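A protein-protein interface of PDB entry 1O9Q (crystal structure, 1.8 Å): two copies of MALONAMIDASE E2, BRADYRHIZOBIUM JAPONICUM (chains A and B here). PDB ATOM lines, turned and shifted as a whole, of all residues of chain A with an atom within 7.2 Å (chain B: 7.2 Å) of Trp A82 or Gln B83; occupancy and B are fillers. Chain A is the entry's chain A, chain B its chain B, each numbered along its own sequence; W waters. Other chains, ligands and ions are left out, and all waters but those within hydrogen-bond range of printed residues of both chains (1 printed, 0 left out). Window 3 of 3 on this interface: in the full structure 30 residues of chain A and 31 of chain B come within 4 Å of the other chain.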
ATOM      1  N   ARG A  41       0.035 -17.355  17.326  1.00  0.00           N
ATOM      2  CA  ARG A  41      -0.129 -18.106  16.088  1.00  0.00           C
ATOM      3  C   ARG A  41       0.723 -17.471  14.999  1.00  0.00           C
ATOM      4  O   ARG A  41       0.839 -16.248  14.906  1.00  0.00           O
ATOM      5  CB  ARG A  41      -1.602 -18.123  15.683  1.00  0.00           C
ATOM      6  CG  ARG A  41      -2.181 -16.770  15.343  1.00  0.00           C
ATOM      7  CD  ARG A  41      -3.693 -16.843  15.236  1.00  0.00           C
ATOM      8  NE  ARG A  41      -4.310 -17.323  16.473  1.00  0.00           N
ATOM      9  CZ  ARG A  41      -4.622 -18.591  16.716  1.00  0.00           C
ATOM     10  NH1 ARG A  41      -4.378 -19.527  15.804  1.00  0.00           N
ATOM     11  NH2 ARG A  41      -5.179 -18.927  17.874  1.00  0.00           N
ATOM     12  N   ASP A  63      -1.898  -9.600  20.050  1.00  0.00           N
ATOM     13  CA  ASP A  63      -3.203 -10.241  19.987  1.00  0.00           C
ATOM     14  C   ASP A  63      -4.451  -9.625  20.648  1.00  0.00           C
ATOM     15  O   ASP A  63      -5.364 -10.355  21.033  1.00  0.00           O
ATOM     16  CB  ASP A  63      -3.041 -11.708  20.406  1.00  0.00           C
ATOM     17  CG  ASP A  63      -4.051 -12.621  19.714  1.00  0.00           C
ATOM     18  OD1 ASP A  63      -4.397 -12.338  18.548  1.00  0.00           O
ATOM     19  OD2 ASP A  63      -4.487 -13.618  20.325  1.00  0.00           O
ATOM     20  N   ASP A  66      -7.534  -6.589  16.397  1.00  0.00           N
ATOM     21  CA  ASP A  66      -8.355  -7.408  15.477  1.00  0.00           C
ATOM     22  C   ASP A  66      -7.752  -7.745  14.116  1.00  0.00           C
ATOM     23  O   ASP A  66      -7.220  -6.875  13.429  1.00  0.00           O
ATOM     24  CB  ASP A  66      -9.698  -6.711  15.217  1.00  0.00           C
ATOM     25  CG  ASP A  66     -10.647  -6.771  16.397  1.00  0.00           C
ATOM     26  OD1 ASP A  66     -10.348  -7.459  17.395  1.00  0.00           O
ATOM     27  OD2 ASP A  66     -11.710  -6.122  16.314  1.00  0.00           O
ATOM     28  N   THR A  67      -7.862  -9.018  13.739  1.00  0.00           N
ATOM     29  CA  THR A  67      -7.416  -9.504  12.423  1.00  0.00           C
ATOM     30  C   THR A  67      -8.585 -10.337  11.885  1.00  0.00           C
ATOM     31  O   THR A  67      -9.225 -11.070  12.640  1.00  0.00           O
ATOM     32  CB  THR A  67      -6.124 -10.375  12.498  1.00  0.00           C
ATOM     33  OG1 THR A  67      -6.226 -11.326  13.566  1.00  0.00           O
ATOM     34  CG2 THR A  67      -4.904  -9.491  12.705  1.00  0.00           C
ATOM     35  N   MET A  70      -7.159 -14.298  11.125  1.00  0.00           N
ATOM     36  CA  MET A  70      -6.562 -15.010  12.266  1.00  0.00           C
ATOM     37  C   MET A  70      -7.318 -14.650  13.535  1.00  0.00           C
ATOM     38  O   MET A  70      -7.787 -13.527  13.682  1.00  0.00           O
ATOM     39  CB  MET A  70      -5.109 -14.577  12.453  1.00  0.00           C
ATOM     40  CG  MET A  70      -4.154 -14.989  11.373  1.00  0.00           C
ATOM     41  SD  MET A  70      -2.507 -14.436  11.832  1.00  0.00           S
ATOM     42  CE  MET A  70      -2.340 -12.993  10.831  1.00  0.00           C
ATOM     43  N   PRO A  71      -7.433 -15.599  14.475  1.00  0.00           N
ATOM     44  CA  PRO A  71      -8.145 -15.295  15.718  1.00  0.00           C
ATOM     45  C   PRO A  71      -7.483 -14.133  16.489  1.00  0.00           C
ATOM     46  O   PRO A  71      -6.321 -13.798  16.257  1.00  0.00           O
ATOM     47  CB  PRO A  71      -8.064 -16.609  16.493  1.00  0.00           C
ATOM     48  CG  PRO A  71      -8.035 -17.648  15.390  1.00  0.00           C
ATOM     49  CD  PRO A  71      -7.074 -17.026  14.401  1.00  0.00           C
ATOM     50  N   THR A  72      -8.243 -13.522  17.387  1.00  0.00           N
ATOM     51  CA  THR A  72      -7.742 -12.423  18.226  1.00  0.00           C
ATOM     52  C   THR A  72      -8.234 -12.831  19.607  1.00  0.00           C
ATOM     53  O   THR A  72      -9.366 -12.534  19.989  1.00  0.00           O
ATOM     54  CB  THR A  72      -8.356 -11.079  17.803  1.00  0.00           C
ATOM     55  OG1 THR A  72      -8.065 -10.838  16.417  1.00  0.00           O
ATOM     56  CG2 THR A  72      -7.779  -9.948  18.642  1.00  0.00           C
ATOM     57  N   GLU A  73      -7.373 -13.525  20.348  1.00  0.00           N
ATOM     58  CA  GLU A  73      -7.750 -14.070  21.658  1.00  0.00           C
ATOM     59  C   GLU A  73      -7.512 -13.235  22.921  1.00  0.00           C
ATOM     60  O   GLU A  73      -7.741 -13.706  24.035  1.00  0.00           O
ATOM     61  CB  GLU A  73      -7.103 -15.454  21.757  1.00  0.00           C
ATOM     62  CG  GLU A  73      -7.433 -16.313  20.536  1.00  0.00           C
ATOM     63  CD  GLU A  73      -6.843 -17.710  20.592  1.00  0.00           C
ATOM     64  OE1 GLU A  73      -5.612 -17.830  20.757  1.00  0.00           O
ATOM     65  OE2 GLU A  73      -7.613 -18.687  20.459  1.00  0.00           O
ATOM     66  N   MET A  74      -7.065 -12.000  22.736  1.00  0.00           N
ATOM     67  CA  MET A  74      -6.857 -11.074  23.861  1.00  0.00           C
ATOM     68  C   MET A  74      -5.976 -11.604  24.997  1.00  0.00           C
ATOM     69  O   MET A  74      -5.948 -11.018  26.082  1.00  0.00           O
ATOM     70  CB  MET A  74      -8.236 -10.712  24.426  1.00  0.00           C
ATOM     71  CG  MET A  74      -9.315 -10.486  23.370  1.00  0.00           C
ATOM     72  SD  MET A  74      -8.934  -9.126  22.260  1.00  0.00           S
ATOM     73  CE  MET A  74     -10.401  -9.133  21.200  1.00  0.00           C
ATOM     74  N   ILE A  78     -11.173 -16.394  27.907  1.00  0.00           N
ATOM     75  CA  ILE A  78     -12.522 -15.898  27.630  1.00  0.00           C
ATOM     76  C   ILE A  78     -12.734 -15.695  26.127  1.00  0.00           C
ATOM     77  O   ILE A  78     -13.851 -15.824  25.626  1.00  0.00           O
ATOM     78  CB  ILE A  78     -12.774 -14.566  28.385  1.00  0.00           C
ATOM     79  CG1 ILE A  78     -12.761 -14.825  29.899  1.00  0.00           C
ATOM     80  CG2 ILE A  78     -14.096 -13.959  27.951  1.00  0.00           C
ATOM     81  CD1 ILE A  78     -12.867 -13.569  30.764  1.00  0.00           C
ATOM     82  N   TYR A  79     -11.656 -15.381  25.415  1.00  0.00           N
ATOM     83  CA  TYR A  79     -11.737 -15.165  23.972  1.00  0.00           C
ATOM     84  C   TYR A  79     -11.029 -16.245  23.150  1.00  0.00           C
ATOM     85  O   TYR A  79     -10.604 -15.994  22.026  1.00  0.00           O
ATOM     86  CB  TYR A  79     -11.159 -13.792  23.629  1.00  0.00           C
ATOM     87  CG  TYR A  79     -12.034 -12.639  24.064  1.00  0.00           C
ATOM     88  CD1 TYR A  79     -12.057 -12.213  25.393  1.00  0.00           C
ATOM     89  CD2 TYR A  79     -12.850 -11.979  23.144  1.00  0.00           C
ATOM     90  CE1 TYR A  79     -12.872 -11.150  25.793  1.00  0.00           C
ATOM     91  CE2 TYR A  79     -13.669 -10.918  23.534  1.00  0.00           C
ATOM     92  CZ  TYR A  79     -13.673 -10.509  24.858  1.00  0.00           C
ATOM     93  OH  TYR A  79     -14.465  -9.444  25.235  1.00  0.00           O
ATOM     94  N   ARG A  80     -10.906 -17.441  23.711  1.00  0.00           N
ATOM     95  CA  ARG A  80     -10.257 -18.543  22.982  1.00  0.00           C
ATOM     96  C   ARG A  80     -11.023 -18.806  21.682  1.00  0.00           C
ATOM     97  O   ARG A  80     -12.241 -18.972  21.694  1.00  0.00           O
ATOM     98  CB  ARG A  80     -10.266 -19.797  23.850  1.00  0.00           C
ATOM     99  CG  ARG A  80      -9.686 -21.026  23.165  1.00  0.00           C
ATOM    100  CD  ARG A  80      -9.925 -22.270  23.997  1.00  0.00           C
ATOM    101  NE  ARG A  80      -9.307 -23.455  23.408  1.00  0.00           N
ATOM    102  CZ  ARG A  80      -9.392 -24.677  23.924  1.00  0.00           C
ATOM    103  NH1 ARG A  80     -10.076 -24.882  25.046  1.00  0.00           N
ATOM    104  NH2 ARG A  80      -8.790 -25.695  23.322  1.00  0.00           N
ATOM    105  N   GLY A  81     -10.304 -18.827  20.567  1.00  0.00           N
ATOM    106  CA  GLY A  81     -10.933 -19.070  19.283  1.00  0.00           C
ATOM    107  C   GLY A  81     -11.733 -17.913  18.700  1.00  0.00           C
ATOM    108  O   GLY A  81     -12.268 -18.035  17.602  1.00  0.00           O
ATOM    109  N   TRP A  82     -11.821 -16.797  19.416  1.00  0.00           N
ATOM    110  CA  TRP A  82     -12.583 -15.627  18.920  1.00  0.00           C
ATOM    111  C   TRP A  82     -12.049 -15.122  17.578  1.00  0.00           C
ATOM    112  O   TRP A  82     -10.851 -14.881  17.424  1.00  0.00           O
ATOM    113  CB  TRP A  82     -12.532 -14.496  19.955  1.00  0.00           C
ATOM    114  CG  TRP A  82     -13.145 -13.211  19.458  1.00  0.00           C
ATOM    115  CD1 TRP A  82     -12.502 -12.021  19.264  1.00  0.00           C
ATOM    116  CD2 TRP A  82     -14.505 -13.002  19.048  1.00  0.00           C
ATOM    117  NE1 TRP A  82     -13.374 -11.087  18.758  1.00  0.00           N
ATOM    118  CE2 TRP A  82     -14.609 -11.661  18.615  1.00  0.00           C
ATOM    119  CE3 TRP A  82     -15.645 -13.819  19.003  1.00  0.00           C
ATOM    120  CZ2 TRP A  82     -15.811 -11.113  18.140  1.00  0.00           C
ATOM    121  CZ3 TRP A  82     -16.844 -13.271  18.528  1.00  0.00           C
ATOM    122  CH2 TRP A  82     -16.912 -11.932  18.105  1.00  0.00           C
ATOM    123  N   GLN A  83     -12.953 -14.949  16.618  1.00  0.00           N
ATOM    124  CA  GLN A  83     -12.563 -14.490  15.283  1.00  0.00           C
ATOM    125  C   GLN A  83     -13.276 -13.212  14.844  1.00  0.00           C
ATOM    126  O   GLN A  83     -14.460 -13.237  14.495  1.00  0.00           O
ATOM    127  CB  GLN A  83     -12.846 -15.615  14.278  1.00  0.00           C
ATOM    128  CG  GLN A  83     -12.424 -15.315  12.846  1.00  0.00           C
ATOM    129  CD  GLN A  83     -10.990 -14.823  12.759  1.00  0.00           C
ATOM    130  OE1 GLN A  83     -10.738 -13.634  12.565  1.00  0.00           O
ATOM    131  NE2 GLN A  83     -10.044 -15.735  12.924  1.00  0.00           N
ATOM    132  N   PRO A  84     -12.558 -12.078  14.853  1.00  0.00           N
ATOM    133  CA  PRO A  84     -13.148 -10.801  14.441  1.00  0.00           C
ATOM    134  C   PRO A  84     -13.541 -10.860  12.961  1.00  0.00           C
ATOM    135  O   PRO A  84     -12.893 -11.542  12.163  1.00  0.00           O
ATOM    136  CB  PRO A  84     -12.019  -9.803  14.684  1.00  0.00           C
ATOM    137  CG  PRO A  84     -11.237 -10.437  15.803  1.00  0.00           C
ATOM    138  CD  PRO A  84     -11.197 -11.877  15.383  1.00  0.00           C
ATOM    139  N   ARG A  85     -14.595 -10.137  12.605  1.00  0.00           N
ATOM    140  CA  ARG A  85     -15.063 -10.101  11.224  1.00  0.00           C
ATOM    141  C   ARG A  85     -14.112  -9.254  10.369  1.00  0.00           C
ATOM    142  O   ARG A  85     -13.870  -9.565   9.205  1.00  0.00           O
ATOM    143  CB  ARG A  85     -16.472  -9.495  11.198  1.00  0.00           C
ATOM    144  CG  ARG A  85     -17.082  -9.311   9.797  1.00  0.00           C
ATOM    145  CD  ARG A  85     -17.643 -10.613   9.220  1.00  0.00           C
ATOM    146  NE  ARG A  85     -18.354 -10.396   7.957  1.00  0.00           N
ATOM    147  CZ  ARG A  85     -17.865 -10.683   6.749  1.00  0.00           C
ATOM    148  NH1 ARG A  85     -16.654 -11.212   6.623  1.00  0.00           N
ATOM    149  NH2 ARG A  85     -18.589 -10.434   5.661  1.00  0.00           N
ATOM    150  N   ARG B  41     -34.090  -6.426  15.540  1.00  0.00           N
ATOM    151  CA  ARG B  41     -34.364  -7.628  16.323  1.00  0.00           C
ATOM    152  C   ARG B  41     -35.044  -7.317  17.658  1.00  0.00           C
ATOM    153  O   ARG B  41     -34.523  -6.558  18.477  1.00  0.00           O
ATOM    154  CB  ARG B  41     -33.043  -8.359  16.577  1.00  0.00           C
ATOM    155  CG  ARG B  41     -32.368  -8.839  15.303  1.00  0.00           C
ATOM    156  CD  ARG B  41     -31.012  -9.454  15.578  1.00  0.00           C
ATOM    157  NE  ARG B  41     -30.325  -9.838  14.348  1.00  0.00           N
ATOM    158  CZ  ARG B  41     -30.794 -10.719  13.471  1.00  0.00           C
ATOM    159  NH1 ARG B  41     -31.966 -11.313  13.685  1.00  0.00           N
ATOM    160  NH2 ARG B  41     -30.085 -11.023  12.388  1.00  0.00           N
ATOM    161  N   ASP B  66     -22.491  -3.009  20.118  1.00  0.00           N
ATOM    162  CA  ASP B  66     -22.338  -4.434  20.454  1.00  0.00           C
ATOM    163  C   ASP B  66     -23.204  -4.998  21.580  1.00  0.00           C
ATOM    164  O   ASP B  66     -23.332  -4.402  22.643  1.00  0.00           O
ATOM    165  CB  ASP B  66     -20.879  -4.722  20.824  1.00  0.00           C
ATOM    166  CG  ASP B  66     -19.947  -4.696  19.632  1.00  0.00           C
ATOM    167  OD1 ASP B  66     -20.426  -4.594  18.483  1.00  0.00           O
ATOM    168  OD2 ASP B  66     -18.722  -4.788  19.862  1.00  0.00           O
ATOM    169  N   THR B  67     -23.778  -6.167  21.325  1.00  0.00           N
ATOM    170  CA  THR B  67     -24.564  -6.898  22.325  1.00  0.00           C
ATOM    171  C   THR B  67     -24.040  -8.326  22.221  1.00  0.00           C
ATOM    172  O   THR B  67     -23.700  -8.782  21.129  1.00  0.00           O
ATOM    173  CB  THR B  67     -26.094  -6.869  22.050  1.00  0.00           C
ATOM    174  OG1 THR B  67     -26.351  -7.006  20.646  1.00  0.00           O
ATOM    175  CG2 THR B  67     -26.700  -5.568  22.570  1.00  0.00           C
ATOM    176  N   ALA B  68     -23.970  -9.022  23.350  1.00  0.00           N
ATOM    177  CA  ALA B  68     -23.450 -10.393  23.369  1.00  0.00           C
ATOM    178  C   ALA B  68     -24.494 -11.483  23.089  1.00  0.00           C
ATOM    179  O   ALA B  68     -24.141 -12.569  22.626  1.00  0.00           O
ATOM    180  CB  ALA B  68     -22.779 -10.664  24.718  1.00  0.00           C
ATOM    181  N   ASN B  69     -25.763 -11.184  23.364  1.00  0.00           N
ATOM    182  CA  ASN B  69     -26.861 -12.159  23.192  1.00  0.00           C
ATOM    183  C   ASN B  69     -27.709 -11.954  21.936  1.00  0.00           C
ATOM    184  O   ASN B  69     -28.571 -12.775  21.623  1.00  0.00           O
ATOM    185  CB  ASN B  69     -27.750 -12.096  24.439  1.00  0.00           C
ATOM    186  CG  ASN B  69     -28.488 -10.777  24.560  1.00  0.00           C
ATOM    187  OD1 ASN B  69     -27.924  -9.707  24.301  1.00  0.00           O
ATOM    188  ND2 ASN B  69     -29.753 -10.840  24.963  1.00  0.00           N
ATOM    189  N   MET B  70     -27.466 -10.851  21.236  1.00  0.00           N
ATOM    190  CA  MET B  70     -28.191 -10.527  20.002  1.00  0.00           C
ATOM    191  C   MET B  70     -27.182 -10.071  18.970  1.00  0.00           C
ATOM    192  O   MET B  70     -26.147  -9.513  19.316  1.00  0.00           O
ATOM    193  CB  MET B  70     -29.170  -9.379  20.248  1.00  0.00           C
ATOM    194  CG  MET B  70     -30.450  -9.768  20.903  1.00  0.00           C
ATOM    195  SD  MET B  70     -31.381  -8.280  21.219  1.00  0.00           S
ATOM    196  CE  MET B  70     -31.273  -8.200  22.992  1.00  0.00           C
ATOM    197  N   PRO B  71     -27.481 -10.292  17.685  1.00  0.00           N
ATOM    198  CA  PRO B  71     -26.572  -9.885  16.612  1.00  0.00           C
ATOM    199  C   PRO B  71     -26.403  -8.352  16.553  1.00  0.00           C
ATOM    200  O   PRO B  71     -27.245  -7.592  17.036  1.00  0.00           O
ATOM    201  CB  PRO B  71     -27.257 -10.428  15.357  1.00  0.00           C
ATOM    202  CG  PRO B  71     -28.014 -11.619  15.862  1.00  0.00           C
ATOM    203  CD  PRO B  71     -28.592 -11.103  17.156  1.00  0.00           C
ATOM    204  N   THR B  72     -25.301  -7.914  15.969  1.00  0.00           N
ATOM    205  CA  THR B  72     -25.036  -6.480  15.800  1.00  0.00           C
ATOM    206  C   THR B  72     -24.623  -6.404  14.334  1.00  0.00           C
ATOM    207  O   THR B  72     -23.461  -6.650  13.991  1.00  0.00           O
ATOM    208  CB  THR B  72     -23.890  -6.015  16.709  1.00  0.00           C
ATOM    209  OG1 THR B  72     -24.198  -6.348  18.068  1.00  0.00           O
ATOM    210  CG2 THR B  72     -23.699  -4.500  16.587  1.00  0.00           C
ATOM    211  N   GLU B  73     -25.588  -6.081  13.473  1.00  0.00           N
ATOM    212  CA  GLU B  73     -25.351  -6.055  12.021  1.00  0.00           C
ATOM    213  C   GLU B  73     -24.955  -4.739  11.347  1.00  0.00           C
ATOM    214  O   GLU B  73     -24.836  -4.687  10.125  1.00  0.00           O
ATOM    215  CB  GLU B  73     -26.583  -6.659  11.341  1.00  0.00           C
ATOM    216  CG  GLU B  73     -26.940  -8.043  11.901  1.00  0.00           C
ATOM    217  CD  GLU B  73     -28.108  -8.692  11.184  1.00  0.00           C
ATOM    218  OE1 GLU B  73     -29.164  -8.035  11.043  1.00  0.00           O
ATOM    219  OE2 GLU B  73     -27.971  -9.865  10.770  1.00  0.00           O
ATOM    220  N   TYR B  79     -22.269  -7.211   7.498  1.00  0.00           N
ATOM    221  CA  TYR B  79     -22.293  -7.769   8.860  1.00  0.00           C
ATOM    222  C   TYR B  79     -23.543  -8.611   9.168  1.00  0.00           C
ATOM    223  O   TYR B  79     -23.943  -8.771  10.330  1.00  0.00           O
ATOM    224  CB  TYR B  79     -22.146  -6.630   9.872  1.00  0.00           C
ATOM    225  CG  TYR B  79     -20.742  -6.070   9.941  1.00  0.00           C
ATOM    226  CD1 TYR B  79     -20.274  -5.175   8.979  1.00  0.00           C
ATOM    227  CD2 TYR B  79     -19.868  -6.467  10.952  1.00  0.00           C
ATOM    228  CE1 TYR B  79     -18.968  -4.690   9.025  1.00  0.00           C
ATOM    229  CE2 TYR B  79     -18.570  -5.994  11.009  1.00  0.00           C
ATOM    230  CZ  TYR B  79     -18.121  -5.106  10.046  1.00  0.00           C
ATOM    231  OH  TYR B  79     -16.830  -4.638  10.123  1.00  0.00           O
ATOM    232  N   ARG B  80     -24.151  -9.158   8.121  1.00  0.00           N
ATOM    233  CA  ARG B  80     -25.337  -9.997   8.301  1.00  0.00           C
ATOM    234  C   ARG B  80     -24.975 -11.156   9.240  1.00  0.00           C
ATOM    235  O   ARG B  80     -24.007 -11.875   9.003  1.00  0.00           O
ATOM    236  CB  ARG B  80     -25.768 -10.548   6.942  1.00  0.00           C
ATOM    237  CG  ARG B  80     -27.019 -11.419   6.991  1.00  0.00           C
ATOM    238  CD  ARG B  80     -28.278 -10.575   7.009  1.00  0.00           C
ATOM    239  NE  ARG B  80     -29.483 -11.399   7.033  1.00  0.00           N
ATOM    240  CZ  ARG B  80     -29.961 -11.996   8.121  1.00  0.00           C
ATOM    241  NH1 ARG B  80     -29.342 -11.860   9.288  1.00  0.00           N
ATOM    242  NH2 ARG B  80     -31.055 -12.743   8.041  1.00  0.00           N
ATOM    243  N   GLY B  81     -25.745 -11.319  10.309  1.00  0.00           N
ATOM    244  CA  GLY B  81     -25.481 -12.395  11.247  1.00  0.00           C
ATOM    245  C   GLY B  81     -24.270 -12.211  12.149  1.00  0.00           C
ATOM    246  O   GLY B  81     -23.924 -13.118  12.902  1.00  0.00           O
ATOM    247  N   TRP B  82     -23.618 -11.053  12.091  1.00  0.00           N
ATOM    248  CA  TRP B  82     -22.442 -10.821  12.947  1.00  0.00           C
ATOM    249  C   TRP B  82     -22.819 -10.830  14.423  1.00  0.00           C
ATOM    250  O   TRP B  82     -23.739 -10.131  14.839  1.00  0.00           O
ATOM    251  CB  TRP B  82     -21.789  -9.477  12.612  1.00  0.00           C
ATOM    252  CG  TRP B  82     -20.640  -9.173  13.538  1.00  0.00           C
ATOM    253  CD1 TRP B  82     -20.542  -8.126  14.412  1.00  0.00           C
ATOM    254  CD2 TRP B  82     -19.460  -9.965  13.728  1.00  0.00           C
ATOM    255  NE1 TRP B  82     -19.374  -8.218  15.134  1.00  0.00           N
ATOM    256  CE2 TRP B  82     -18.692  -9.338  14.735  1.00  0.00           C
ATOM    257  CE3 TRP B  82     -18.979 -11.149  13.147  1.00  0.00           C
ATOM    258  CZ2 TRP B  82     -17.463  -9.854  15.177  1.00  0.00           C
ATOM    259  CZ3 TRP B  82     -17.756 -11.664  13.589  1.00  0.00           C
ATOM    260  CH2 TRP B  82     -17.015 -11.016  14.594  1.00  0.00           C
ATOM    261  N   GLN B  83     -22.099 -11.620  15.212  1.00  0.00           N
ATOM    262  CA  GLN B  83     -22.375 -11.708  16.640  1.00  0.00           C
ATOM    263  C   GLN B  83     -21.175 -11.327  17.510  1.00  0.00           C
ATOM    264  O   GLN B  83     -20.201 -12.076  17.607  1.00  0.00           O
ATOM    265  CB  GLN B  83     -22.831 -13.136  16.965  1.00  0.00           C
ATOM    266  CG  GLN B  83     -23.160 -13.356  18.426  1.00  0.00           C
ATOM    267  CD  GLN B  83     -24.126 -12.317  18.958  1.00  0.00           C
ATOM    268  OE1 GLN B  83     -23.741 -11.420  19.712  1.00  0.00           O
ATOM    269  NE2 GLN B  83     -25.386 -12.425  18.560  1.00  0.00           N
ATOM    270  N   PRO B  84     -21.221 -10.134  18.128  1.00  0.00           N
ATOM    271  CA  PRO B  84     -20.124  -9.687  18.991  1.00  0.00           C
ATOM    272  C   PRO B  84     -19.977 -10.645  20.177  1.00  0.00           C
ATOM    273  O   PRO B  84     -20.952 -11.262  20.607  1.00  0.00           O
ATOM    274  CB  PRO B  84     -20.579  -8.297  19.435  1.00  0.00           C
ATOM    275  CG  PRO B  84     -21.337  -7.801  18.240  1.00  0.00           C
ATOM    276  CD  PRO B  84     -22.150  -9.024  17.841  1.00  0.00           C
ATOM    277  N   ARG B  85     -18.761 -10.770  20.695  1.00  0.00           N
ATOM    278  CA  ARG B  85     -18.512 -11.652  21.844  1.00  0.00           C
ATOM    279  C   ARG B  85     -19.018 -11.015  23.139  1.00  0.00           C
ATOM    280  O   ARG B  85     -19.580 -11.692  23.999  1.00  0.00           O
ATOM    281  CB  ARG B  85     -17.007 -11.918  21.946  1.00  0.00           C
ATOM    282  CG  ARG B  85     -16.567 -12.708  23.179  1.00  0.00           C
ATOM    283  CD  ARG B  85     -17.244 -14.066  23.295  1.00  0.00           C
ATOM    284  NE  ARG B  85     -16.619 -14.906  24.319  1.00  0.00           N
ATOM    285  CZ  ARG B  85     -17.287 -15.633  25.211  1.00  0.00           C
ATOM    286  NH1 ARG B  85     -18.616 -15.629  25.219  1.00  0.00           N
ATOM    287  NH2 ARG B  85     -16.628 -16.372  26.097  1.00  0.00           N
ATOM    288  N   SER B  86     -18.839  -9.704  23.257  1.00  0.00           N
ATOM    289  CA  SER B  86     -19.235  -8.986  24.475  1.00  0.00           C
ATOM    290  C   SER B  86     -20.240  -7.850  24.280  1.00  0.00           C
ATOM    291  O   SER B  86     -20.433  -7.348  23.168  1.00  0.00           O
ATOM    292  CB  SER B  86     -17.970  -8.413  25.104  1.00  0.00           C
ATOM    293  OG  SER B  86     -17.297  -7.570  24.178  1.00  0.00           O
ATOM    294  N   ASP B  87     -20.879  -7.465  25.380  1.00  0.00           N
ATOM    295  CA  ASP B  87     -21.827  -6.349  25.374  1.00  0.00           C
ATOM    296  C   ASP B  87     -20.960  -5.091  25.462  1.00  0.00           C
ATOM    297  O   ASP B  87     -19.966  -5.071  26.187  1.00  0.00           O
ATOM    298  CB  ASP B  87     -22.732  -6.427  26.608  1.00  0.00           C
ATOM    299  CG  ASP B  87     -23.810  -7.487  26.479  1.00  0.00           C
ATOM    300  OD1 ASP B  87     -24.495  -7.506  25.435  1.00  0.00           O
ATOM    301  OD2 ASP B  87     -23.979  -8.294  27.422  1.00  0.00           O
HETATM  302  O   HOH W   1     -20.969 -11.099   9.104  1.00  0.00           O
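O of Ile A78 is in hydrogen-bond range of NH2 of Arg B85 (2.9 Å).
The backbone carbonyl oxygen (O) of Thr A67 lies close to the side-chain amide oxygen (OE1) of Gln A83.
OE1 of Gln A83 lies close to O of Met A70, at 3.2 Å.
The backbone carbonyl oxygen (O) of Trp A82 is in hydrogen-bond range of the backbone NH (N) of Thr A72 (2.9 Å).
The backbone carbonyl oxygen of Thr B67 lies close to the side-chain amide oxygen of Gln B83 (3.0 Å).
The backbone carbonyl oxygen (O) of Ala B68 lies close to the side-chain amide oxygen (OE1) of Gln B83, at 3.2 Å.
The backbone carbonyl oxygen (O) of Met B70 sits close to the side-chain amide oxygen (OE1) of Gln B83 (3.1 Å).
Tyr A79 touches Arg B85 (CE2 to CG, 3.4 Å).
OH of Tyr A79 touches OG of Ser B86, 3.6 Å away.
Trp A82 touches Trp B82.
Trp A82 touches Gln B83 (CH2 to O, 3.3 Å).
Trp A82 touches Pro B84 (CH2 to C, 3.9 Å).
Arg B85 touches Trp A82.
Gln A83 touches Trp B82 (O to CH2, 3.4 Å).
CH2 of Trp B82 touches C of Pro A84, at 3.8 Å.
Arg A85 touches Tyr B79 (CG to CE2, 3.8 Å).
CH2 of Trp B82 touches N of Arg A85 (3.3 Å).
Met A70 touches none of the printed residues of chain B.
Of the printed residues of chain B, Ile A78 touches Arg B85.
Of the printed residues of chain B, Tyr A79 touches Arg B85 (3.4 Å) and Ser B86 (3.6 Å).
Arg A80 touches none of the printed residues of chain B.
No residue of chain B comes within 4 Å of Gly A81.
Of the printed residues of chain B, Trp A82 touches Trp B82 (3.6 Å), Gln B83 (3.3 Å), Pro B84 (3.9 Å) and Arg B85 (3.4 Å).
Of the printed residues of chain A, Tyr B79 touches Arg A85.
Of the printed residues of chain A, Trp B82 touches Trp A82 (3.6 Å), Gln A83 (3.4 Å), Pro A84 (3.8 Å) and Arg A85 (3.3 Å).
Gln B83 touches just one residue of chain A: Trp A82 (3.3 Å).
Of the printed residues of chain A, Arg B85 touches Ile A78 (2.9 Å), Tyr A79 (3.4 Å) and Trp A82 (3.4 Å).
The nearest residue of chain B that does not touch Trp A82 is Ser B86 (5.9 Å).
The nearest residue of chain A that does not touch Gln B83 is Gln A83 (6.6 Å).
The nearest printed residue of chain B that does not touch Gln A83 is Gln B83 (6.6 Å).
Of the 17 printed residues of chain A, 6 touch a printed residue of chain B.
Printed residues of chain A that touch a printed residue of chain B: Ile A78, Tyr A79, Trp A82, Gln A83, Pro A84 and Arg A85.
Hydrophobic or aromatic side chains of chain A within 4 Å of the printed part of chain B: Ile A78, Tyr A79 and Trp A82.
Among the printed residues, 11 pairs touch across the chains.
Among the printed residues, no Asp or Glu carboxylate lies within 4 Å of a Lys or Arg side-chain nitrogen of the other chain.
Trp A82 touches its own counterpart, Trp B82.
Trp A82 touches Gln B83, and with the chains exchanged Gln A83 touches Trp B82.
Trp A82 touches Pro B84, and with the chains exchanged Pro A84 touches Trp B82.
Trp A82 touches Arg B85, and with the chains exchanged Arg A85 touches Trp B82.
Of the 11 pairs that touch across the chains among the printed residues, 9 have their exchanged pair printed and touching as well.
Water W1 bridges the guanidinium group of Arg A85 and the backbone carbonyl oxygen of Arg B80.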
